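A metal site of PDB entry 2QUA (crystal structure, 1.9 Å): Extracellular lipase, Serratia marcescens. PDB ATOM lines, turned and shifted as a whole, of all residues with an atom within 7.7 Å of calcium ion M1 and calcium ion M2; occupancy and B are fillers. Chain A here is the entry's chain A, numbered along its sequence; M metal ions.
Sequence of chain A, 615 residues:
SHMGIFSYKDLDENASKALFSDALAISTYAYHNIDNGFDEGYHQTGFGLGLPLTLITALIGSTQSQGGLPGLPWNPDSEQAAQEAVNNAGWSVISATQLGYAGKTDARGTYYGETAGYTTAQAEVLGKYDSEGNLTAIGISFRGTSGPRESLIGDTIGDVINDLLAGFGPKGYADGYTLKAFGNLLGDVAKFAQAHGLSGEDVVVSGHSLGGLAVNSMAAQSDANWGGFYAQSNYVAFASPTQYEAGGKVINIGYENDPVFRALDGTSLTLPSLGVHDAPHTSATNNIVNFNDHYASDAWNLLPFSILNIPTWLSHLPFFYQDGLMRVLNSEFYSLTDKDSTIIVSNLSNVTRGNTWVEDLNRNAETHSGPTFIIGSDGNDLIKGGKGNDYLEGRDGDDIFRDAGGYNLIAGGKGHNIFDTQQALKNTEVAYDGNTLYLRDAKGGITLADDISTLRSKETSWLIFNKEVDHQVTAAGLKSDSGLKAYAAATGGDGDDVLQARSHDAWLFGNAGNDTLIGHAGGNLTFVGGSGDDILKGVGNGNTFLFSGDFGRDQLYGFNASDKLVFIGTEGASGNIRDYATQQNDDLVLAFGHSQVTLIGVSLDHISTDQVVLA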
ATOM      1  N   SER A 346      20.563  10.326  -2.567  1.00  0.00           N
ATOM      2  CA  SER A 346      21.569  11.225  -3.084  1.00  0.00           C
ATOM      3  C   SER A 346      22.987  10.845  -2.644  1.00  0.00           C
ATOM      4  O   SER A 346      23.280  10.825  -1.451  1.00  0.00           O
ATOM      5  CB  SER A 346      21.263  12.680  -2.669  1.00  0.00           C
ATOM      6  OG  SER A 346      22.314  13.527  -3.091  1.00  0.00           O
ATOM      7  N   ARG A 353      27.018  17.929  -7.391  1.00  0.00           N
ATOM      8  CA  ARG A 353      25.881  18.150  -6.464  1.00  0.00           C
ATOM      9  C   ARG A 353      25.188  19.481  -6.755  1.00  0.00           C
ATOM     10  O   ARG A 353      23.969  19.586  -6.633  1.00  0.00           O
ATOM     11  CB  ARG A 353      26.295  18.073  -4.987  1.00  0.00           C
ATOM     12  CG  ARG A 353      25.101  17.946  -3.973  1.00  0.00           C
ATOM     13  CD  ARG A 353      25.597  17.762  -2.495  1.00  0.00           C
ATOM     14  NE  ARG A 353      26.541  16.636  -2.374  1.00  0.00           N
ATOM     15  CZ  ARG A 353      27.852  16.761  -2.184  1.00  0.00           C
ATOM     16  NH1 ARG A 353      28.414  17.974  -2.072  1.00  0.00           N
ATOM     17  NH2 ARG A 353      28.617  15.674  -2.106  1.00  0.00           N
ATOM     18  N   ILE A 375      15.970  11.062  -0.689  1.00  0.00           N
ATOM     19  CA  ILE A 375      16.761  11.368   0.512  1.00  0.00           C
ATOM     20  C   ILE A 375      17.991  12.181   0.193  1.00  0.00           C
ATOM     21  O   ILE A 375      18.898  11.664  -0.466  1.00  0.00           O
ATOM     22  CB  ILE A 375      17.261  10.069   1.202  1.00  0.00           C
ATOM     23  CG1 ILE A 375      16.131   9.042   1.373  1.00  0.00           C
ATOM     24  CG2 ILE A 375      17.929  10.396   2.525  1.00  0.00           C
ATOM     25  CD1 ILE A 375      14.965   9.565   2.169  1.00  0.00           C
ATOM     26  N   GLY A 376      18.025  13.435   0.683  1.00  0.00           N
ATOM     27  CA  GLY A 376      19.138  14.353   0.413  1.00  0.00           C
ATOM     28  C   GLY A 376      20.393  13.982   1.181  1.00  0.00           C
ATOM     29  O   GLY A 376      20.490  12.922   1.791  1.00  0.00           O
ATOM     30  N   SER A 377      21.372  14.876   1.145  1.00  0.00           N
ATOM     31  CA  SER A 377      22.607  14.664   1.841  1.00  0.00           C
ATOM     32  C   SER A 377      22.714  15.817   2.836  1.00  0.00           C
ATOM     33  O   SER A 377      21.884  16.759   2.822  1.00  0.00           O
ATOM     34  CB  SER A 377      23.775  14.709   0.832  1.00  0.00           C
ATOM     35  OG  SER A 377      24.096  16.070   0.553  1.00  0.00           O
ATOM     36  N   ASP A 378      23.715  15.781   3.705  1.00  0.00           N
ATOM     37  CA  ASP A 378      23.892  16.935   4.587  1.00  0.00           C
ATOM     38  C   ASP A 378      24.557  18.125   3.873  1.00  0.00           C
ATOM     39  O   ASP A 378      24.838  19.132   4.495  1.00  0.00           O
ATOM     40  CB  ASP A 378      24.629  16.530   5.864  1.00  0.00           C
ATOM     41  CG  ASP A 378      23.731  15.710   6.801  1.00  0.00           C
ATOM     42  OD1 ASP A 378      22.508  15.989   6.850  1.00  0.00           O
ATOM     43  OD2 ASP A 378      24.244  14.810   7.470  1.00  0.00           O
ATOM     44  N   GLY A 379      24.782  17.994   2.563  1.00  0.00           N
ATOM     45  CA  GLY A 379      25.239  19.133   1.761  1.00  0.00           C
ATOM     46  C   GLY A 379      24.063  19.855   1.102  1.00  0.00           C
ATOM     47  O   GLY A 379      22.893  19.549   1.368  1.00  0.00           O
ATOM     48  N   ASN A 380      24.375  20.835   0.261  1.00  0.00           N
ATOM     49  CA  ASN A 380      23.400  21.590  -0.501  1.00  0.00           C
ATOM     50  C   ASN A 380      22.915  20.789  -1.702  1.00  0.00           C
ATOM     51  O   ASN A 380      23.665  20.550  -2.657  1.00  0.00           O
ATOM     52  CB  ASN A 380      24.023  22.892  -1.021  1.00  0.00           C
ATOM     53  CG  ASN A 380      24.438  23.813   0.096  1.00  0.00           C
ATOM     54  OD1 ASN A 380      24.184  23.549   1.280  1.00  0.00           O
ATOM     55  ND2 ASN A 380      25.072  24.906  -0.262  1.00  0.00           N
ATOM     56  N   ASP A 381      21.652  20.375  -1.646  1.00  0.00           N
ATOM     57  CA  ASP A 381      21.087  19.484  -2.665  1.00  0.00           C
ATOM     58  C   ASP A 381      20.141  20.179  -3.642  1.00  0.00           C
ATOM     59  O   ASP A 381      19.545  21.215  -3.304  1.00  0.00           O
ATOM     60  CB  ASP A 381      20.332  18.326  -1.981  1.00  0.00           C
ATOM     61  CG  ASP A 381      21.209  17.561  -1.009  1.00  0.00           C
ATOM     62  OD1 ASP A 381      22.300  17.106  -1.475  1.00  0.00           O
ATOM     63  OD2 ASP A 381      20.817  17.411   0.191  1.00  0.00           O
ATOM     64  N   LEU A 382      20.036  19.599  -4.837  1.00  0.00           N
ATOM     65  CA  LEU A 382      19.008  19.915  -5.827  1.00  0.00           C
ATOM     66  C   LEU A 382      18.183  18.641  -5.942  1.00  0.00           C
ATOM     67  O   LEU A 382      18.651  17.614  -6.429  1.00  0.00           O
ATOM     68  CB  LEU A 382      19.596  20.306  -7.187  1.00  0.00           C
ATOM     69  CG  LEU A 382      20.652  21.413  -7.210  1.00  0.00           C
ATOM     70  CD1 LEU A 382      21.137  21.700  -8.657  1.00  0.00           C
ATOM     71  CD2 LEU A 382      20.151  22.701  -6.506  1.00  0.00           C
ATOM     72  N   ILE A 383      16.941  18.710  -5.482  1.00  0.00           N
ATOM     73  CA  ILE A 383      16.107  17.539  -5.363  1.00  0.00           C
ATOM     74  C   ILE A 383      14.820  17.747  -6.169  1.00  0.00           C
ATOM     75  O   ILE A 383      14.151  18.762  -5.978  1.00  0.00           O
ATOM     76  CB  ILE A 383      15.787  17.304  -3.864  1.00  0.00           C
ATOM     77  CG1 ILE A 383      17.081  16.938  -3.108  1.00  0.00           C
ATOM     78  CG2 ILE A 383      14.714  16.194  -3.677  1.00  0.00           C
ATOM     79  CD1 ILE A 383      16.870  16.795  -1.577  1.00  0.00           C
ATOM     80  N   GLU A 393      13.332  14.807   1.246  1.00  0.00           N
ATOM     81  CA  GLU A 393      13.985  15.142   2.506  1.00  0.00           C
ATOM     82  C   GLU A 393      15.305  15.828   2.233  1.00  0.00           C
ATOM     83  O   GLU A 393      16.231  15.216   1.705  1.00  0.00           O
ATOM     84  CB  GLU A 393      14.224  13.883   3.349  1.00  0.00           C
ATOM     85  CG  GLU A 393      14.707  14.211   4.746  1.00  0.00           C
ATOM     86  CD  GLU A 393      14.903  12.988   5.608  1.00  0.00           C
ATOM     87  OE1 GLU A 393      15.094  11.889   5.039  1.00  0.00           O
ATOM     88  OE2 GLU A 393      14.883  13.111   6.855  1.00  0.00           O
ATOM     89  N   GLY A 394      15.397  17.107   2.587  1.00  0.00           N
ATOM     90  CA  GLY A 394      16.661  17.830   2.371  1.00  0.00           C
ATOM     91  C   GLY A 394      17.818  17.511   3.317  1.00  0.00           C
ATOM     92  O   GLY A 394      18.973  17.529   2.895  1.00  0.00           O
ATOM     93  N   ARG A 395      17.520  17.217   4.586  1.00  0.00           N
ATOM     94  CA  ARG A 395      18.533  17.156   5.641  1.00  0.00           C
ATOM     95  C   ARG A 395      19.281  18.519   5.731  1.00  0.00           C
ATOM     96  O   ARG A 395      18.784  19.535   5.266  1.00  0.00           O
ATOM     97  CB  ARG A 395      19.507  15.963   5.442  1.00  0.00           C
ATOM     98  CG  ARG A 395      18.810  14.587   5.330  1.00  0.00           C
ATOM     99  CD  ARG A 395      19.833  13.439   5.248  1.00  0.00           C
ATOM    100  NE  ARG A 395      20.896  13.594   6.233  1.00  0.00           N
ATOM    101  CZ  ARG A 395      20.944  12.992   7.422  1.00  0.00           C
ATOM    102  NH1 ARG A 395      19.968  12.164   7.807  1.00  0.00           N
ATOM    103  NH2 ARG A 395      21.967  13.219   8.227  1.00  0.00           N
ATOM    104  N   ASP A 396      20.465  18.516   6.337  1.00  0.00           N
ATOM    105  CA  ASP A 396      21.262  19.736   6.506  1.00  0.00           C
ATOM    106  C   ASP A 396      21.629  20.329   5.147  1.00  0.00           C
ATOM    107  O   ASP A 396      21.439  19.714   4.096  1.00  0.00           O
ATOM    108  CB  ASP A 396      22.554  19.467   7.292  1.00  0.00           C
ATOM    109  CG  ASP A 396      22.306  19.115   8.750  1.00  0.00           C
ATOM    110  OD1 ASP A 396      21.135  18.899   9.148  1.00  0.00           O
ATOM    111  OD2 ASP A 396      23.311  19.045   9.510  1.00  0.00           O
ATOM    112  N   GLY A 397      22.167  21.542   5.199  1.00  0.00           N
ATOM    113  CA  GLY A 397      22.546  22.224   3.978  1.00  0.00           C
ATOM    114  C   GLY A 397      21.380  22.979   3.390  1.00  0.00           C
ATOM    115  O   GLY A 397      20.202  22.763   3.726  1.00  0.00           O
ATOM    116  N   ASP A 398      21.727  23.900   2.486  1.00  0.00           N
ATOM    117  CA  ASP A 398      20.778  24.748   1.791  1.00  0.00           C
ATOM    118  C   ASP A 398      20.283  24.009   0.550  1.00  0.00           C
ATOM    119  O   ASP A 398      20.980  23.879  -0.447  1.00  0.00           O
ATOM    120  CB  ASP A 398      21.460  26.066   1.399  1.00  0.00           C
ATOM    121  CG  ASP A 398      21.970  26.848   2.597  1.00  0.00           C
ATOM    122  OD1 ASP A 398      21.553  26.596   3.742  1.00  0.00           O
ATOM    123  OD2 ASP A 398      22.786  27.765   2.385  1.00  0.00           O
ATOM    124  N   ASP A 399      19.046  23.525   0.619  1.00  0.00           N
ATOM    125  CA  ASP A 399      18.521  22.644  -0.400  1.00  0.00           C
ATOM    126  C   ASP A 399      17.487  23.350  -1.261  1.00  0.00           C
ATOM    127  O   ASP A 399      16.792  24.264  -0.781  1.00  0.00           O
ATOM    128  CB  ASP A 399      17.930  21.392   0.296  1.00  0.00           C
ATOM    129  CG  ASP A 399      18.986  20.632   1.101  1.00  0.00           C
ATOM    130  OD1 ASP A 399      20.055  20.325   0.537  1.00  0.00           O
ATOM    131  OD2 ASP A 399      18.799  20.308   2.299  1.00  0.00           O
ATOM    132  N   ILE A 400      17.402  22.940  -2.527  1.00  0.00           N
ATOM    133  CA  ILE A 400      16.345  23.443  -3.441  1.00  0.00           C
ATOM    134  C   ILE A 400      15.516  22.257  -3.921  1.00  0.00           C
ATOM    135  O   ILE A 400      16.082  21.264  -4.383  1.00  0.00           O
ATOM    136  CB  ILE A 400      16.903  24.268  -4.640  1.00  0.00           C
ATOM    137  CG1 ILE A 400      17.867  25.345  -4.154  1.00  0.00           C
ATOM    138  CG2 ILE A 400      15.734  24.907  -5.472  1.00  0.00           C
ATOM    139  CD1 ILE A 400      18.555  26.160  -5.251  1.00  0.00           C
ATOM    140  N   PHE A 401      14.186  22.371  -3.788  1.00  0.00           N
ATOM    141  CA  PHE A 401      13.245  21.391  -4.278  1.00  0.00           C
ATOM    142  C   PHE A 401      12.423  21.880  -5.447  1.00  0.00           C
ATOM    143  O   PHE A 401      12.007  23.061  -5.502  1.00  0.00           O
ATOM    144  CB  PHE A 401      12.265  21.013  -3.174  1.00  0.00           C
ATOM    145  CG  PHE A 401      12.942  20.578  -1.935  1.00  0.00           C
ATOM    146  CD1 PHE A 401      13.195  19.226  -1.690  1.00  0.00           C
ATOM    147  CD2 PHE A 401      13.352  21.512  -1.015  1.00  0.00           C
ATOM    148  CE1 PHE A 401      13.849  18.815  -0.527  1.00  0.00           C
ATOM    149  CE2 PHE A 401      14.030  21.115   0.163  1.00  0.00           C
ATOM    150  CZ  PHE A 401      14.262  19.764   0.386  1.00  0.00           C
ATOM    151  N   ALA A 411      10.474  17.910   3.515  1.00  0.00           N
ATOM    152  CA  ALA A 411      11.146  18.309   4.739  1.00  0.00           C
ATOM    153  C   ALA A 411      12.455  19.038   4.412  1.00  0.00           C
ATOM    154  O   ALA A 411      13.489  18.411   4.158  1.00  0.00           O
ATOM    155  CB  ALA A 411      11.418  17.093   5.609  1.00  0.00           C
ATOM    156  N   GLY A 412      12.415  20.374   4.428  1.00  0.00           N
ATOM    157  CA  GLY A 412      13.619  21.163   4.113  1.00  0.00           C
ATOM    158  C   GLY A 412      14.798  20.823   5.019  1.00  0.00           C
ATOM    159  O   GLY A 412      15.977  20.893   4.598  1.00  0.00           O
ATOM    160  N   GLY A 413      14.493  20.453   6.259  1.00  0.00           N
ATOM    161  CA  GLY A 413      15.529  20.237   7.262  1.00  0.00           C
ATOM    162  C   GLY A 413      16.224  21.532   7.645  1.00  0.00           C
ATOM    163  O   GLY A 413      15.696  22.642   7.411  1.00  0.00           O
ATOM    164  N   LYS A 414      17.412  21.425   8.232  1.00  0.00           N
ATOM    165  CA  LYS A 414      18.185  22.642   8.504  1.00  0.00           C
ATOM    166  C   LYS A 414      18.604  23.392   7.237  1.00  0.00           C
ATOM    167  O   LYS A 414      18.517  22.869   6.110  1.00  0.00           O
ATOM    168  CB  LYS A 414      19.441  22.321   9.328  1.00  0.00           C
ATOM    169  CG  LYS A 414      19.144  21.872  10.731  1.00  0.00           C
ATOM    170  CD  LYS A 414      20.428  21.517  11.460  1.00  0.00           C
ATOM    171  CE  LYS A 414      20.094  20.923  12.803  1.00  0.00           C
ATOM    172  NZ  LYS A 414      21.321  20.637  13.561  1.00  0.00           N
ATOM    173  N   GLY A 415      19.071  24.618   7.449  1.00  0.00           N
ATOM    174  CA  GLY A 415      19.627  25.426   6.372  1.00  0.00           C
ATOM    175  C   GLY A 415      18.598  26.354   5.764  1.00  0.00           C
ATOM    176  O   GLY A 415      17.463  26.480   6.247  1.00  0.00           O
ATOM    177  N   HIS A 416      19.019  27.018   4.701  1.00  0.00           N
ATOM    178  CA  HIS A 416      18.149  27.921   3.978  1.00  0.00           C
ATOM    179  C   HIS A 416      17.608  27.145   2.763  1.00  0.00           C
ATOM    180  O   HIS A 416      18.321  26.911   1.801  1.00  0.00           O
ATOM    181  CB  HIS A 416      18.904  29.185   3.557  1.00  0.00           C
ATOM    182  CG  HIS A 416      18.052  30.151   2.798  1.00  0.00           C
ATOM    183  ND1 HIS A 416      17.608  31.338   3.340  1.00  0.00           N
ATOM    184  CD2 HIS A 416      17.559  30.105   1.531  1.00  0.00           C
ATOM    185  CE1 HIS A 416      16.870  31.977   2.442  1.00  0.00           C
ATOM    186  NE2 HIS A 416      16.821  31.253   1.342  1.00  0.00           N
ATOM    187  N   ASN A 417      16.339  26.744   2.830  1.00  0.00           N
ATOM    188  CA  ASN A 417      15.796  25.861   1.813  1.00  0.00           C
ATOM    189  C   ASN A 417      14.807  26.555   0.916  1.00  0.00           C
ATOM    190  O   ASN A 417      14.040  27.406   1.381  1.00  0.00           O
ATOM    191  CB  ASN A 417      15.146  24.624   2.469  1.00  0.00           C
ATOM    192  CG  ASN A 417      16.040  23.987   3.510  1.00  0.00           C
ATOM    193  OD1 ASN A 417      17.138  23.480   3.210  1.00  0.00           O
ATOM    194  ND2 ASN A 417      15.577  24.003   4.761  1.00  0.00           N
ATOM    195  N   ILE A 418      14.853  26.210  -0.371  1.00  0.00           N
ATOM    196  CA  ILE A 418      14.006  26.857  -1.396  1.00  0.00           C
ATOM    197  C   ILE A 418      13.063  25.829  -2.011  1.00  0.00           C
ATOM    198  O   ILE A 418      13.458  24.672  -2.286  1.00  0.00           O
ATOM    199  CB  ILE A 418      14.879  27.538  -2.488  1.00  0.00           C
ATOM    200  CG1 ILE A 418      15.776  28.625  -1.863  1.00  0.00           C
ATOM    201  CG2 ILE A 418      13.997  28.125  -3.624  1.00  0.00           C
ATOM    202  CD1 ILE A 418      16.913  29.078  -2.740  1.00  0.00           C
ATOM    203  N   ASP A 451      10.142  24.011   6.759  1.00  0.00           N
ATOM    204  CA  ASP A 451      11.463  24.664   6.723  1.00  0.00           C
ATOM    205  C   ASP A 451      11.866  25.252   5.371  1.00  0.00           C
ATOM    206  O   ASP A 451      13.044  25.203   4.983  1.00  0.00           O
ATOM    207  CB  ASP A 451      12.548  23.712   7.230  1.00  0.00           C
ATOM    208  CG  ASP A 451      12.319  23.353   8.698  1.00  0.00           C
ATOM    209  OD1 ASP A 451      12.224  24.280   9.539  1.00  0.00           O
ATOM    210  OD2 ASP A 451      12.203  22.160   8.993  1.00  0.00           O
HETATM  211 CA    CA M   1      20.797  18.745   2.109  1.00  0.00          CA
HETATM  212 CA    CA M   2      18.219  21.575   4.212  1.00  0.00          CA
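OD1 of Asp 378 sits at hydrogen-bond distance from N of Asp 396.
The backbone NH of Gly 394 lies within hydrogen-bond range of the backbone carbonyl oxygen of Ala 411, at 2.8 Å.
O of Asp 381 sits at hydrogen-bond distance from N of Ile 400.
The backbone carbonyl oxygen of Asp 399 lies within hydrogen-bond range of the backbone NH of Ile 418, at 2.8 Å.
The side-chain hydroxyl of Ser 377 lies within hydrogen-bond range of the backbone NH of Gly 379 (2.9 Å).
The side-chain amide nitrogen of Asn 417 lies within hydrogen-bond range of the backbone carbonyl oxygen of Gly 413, 3.0 Å away.
ND2 of Asn 417 is in hydrogen-bond range of O of Gly 415, 3.4 Å away.
The side-chain amide nitrogen (ND2) of Asn 417 is in hydrogen-bond range of the backbone carbonyl oxygen (O) of Asp 451 (2.8 Å).
C of Gly 413 touches calcium ion M2 (3.97 Å).
Eight residues have an atom within 4 Å of calcium ion M2: Arg 395, Asp 396, Gly 397, Asp 399, Gly 412, Gly 413, Lys 414 and Asn 417.
Calcium ion M1 is bound by O of Asp 396 (2.3 Å), O of Gly 394 (2.3 Å), OD2 of Asp 381 (2.3 Å), OD1 of Asp 399 (2.3 Å), O of Gly 379 (2.4 Å), O of Ser 377 (2.4 Å) and OD2 of Asp 399 (2.5 Å).
Calcium ion M2 is bound by the backbone carbonyl oxygen (O) of Lys 414 (2.3 Å), the backbone carbonyl oxygen (O) of Gly 397 (2.4 Å), the backbone carbonyl oxygen (O) of Arg 395 (2.4 Å), the side-chain carboxylate (OD2) of Asp 399 (2.4 Å), the backbone carbonyl oxygen (O) of Gly 412 (2.4 Å) and the side-chain amide oxygen (OD1) of Asn 417 (2.4 Å).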
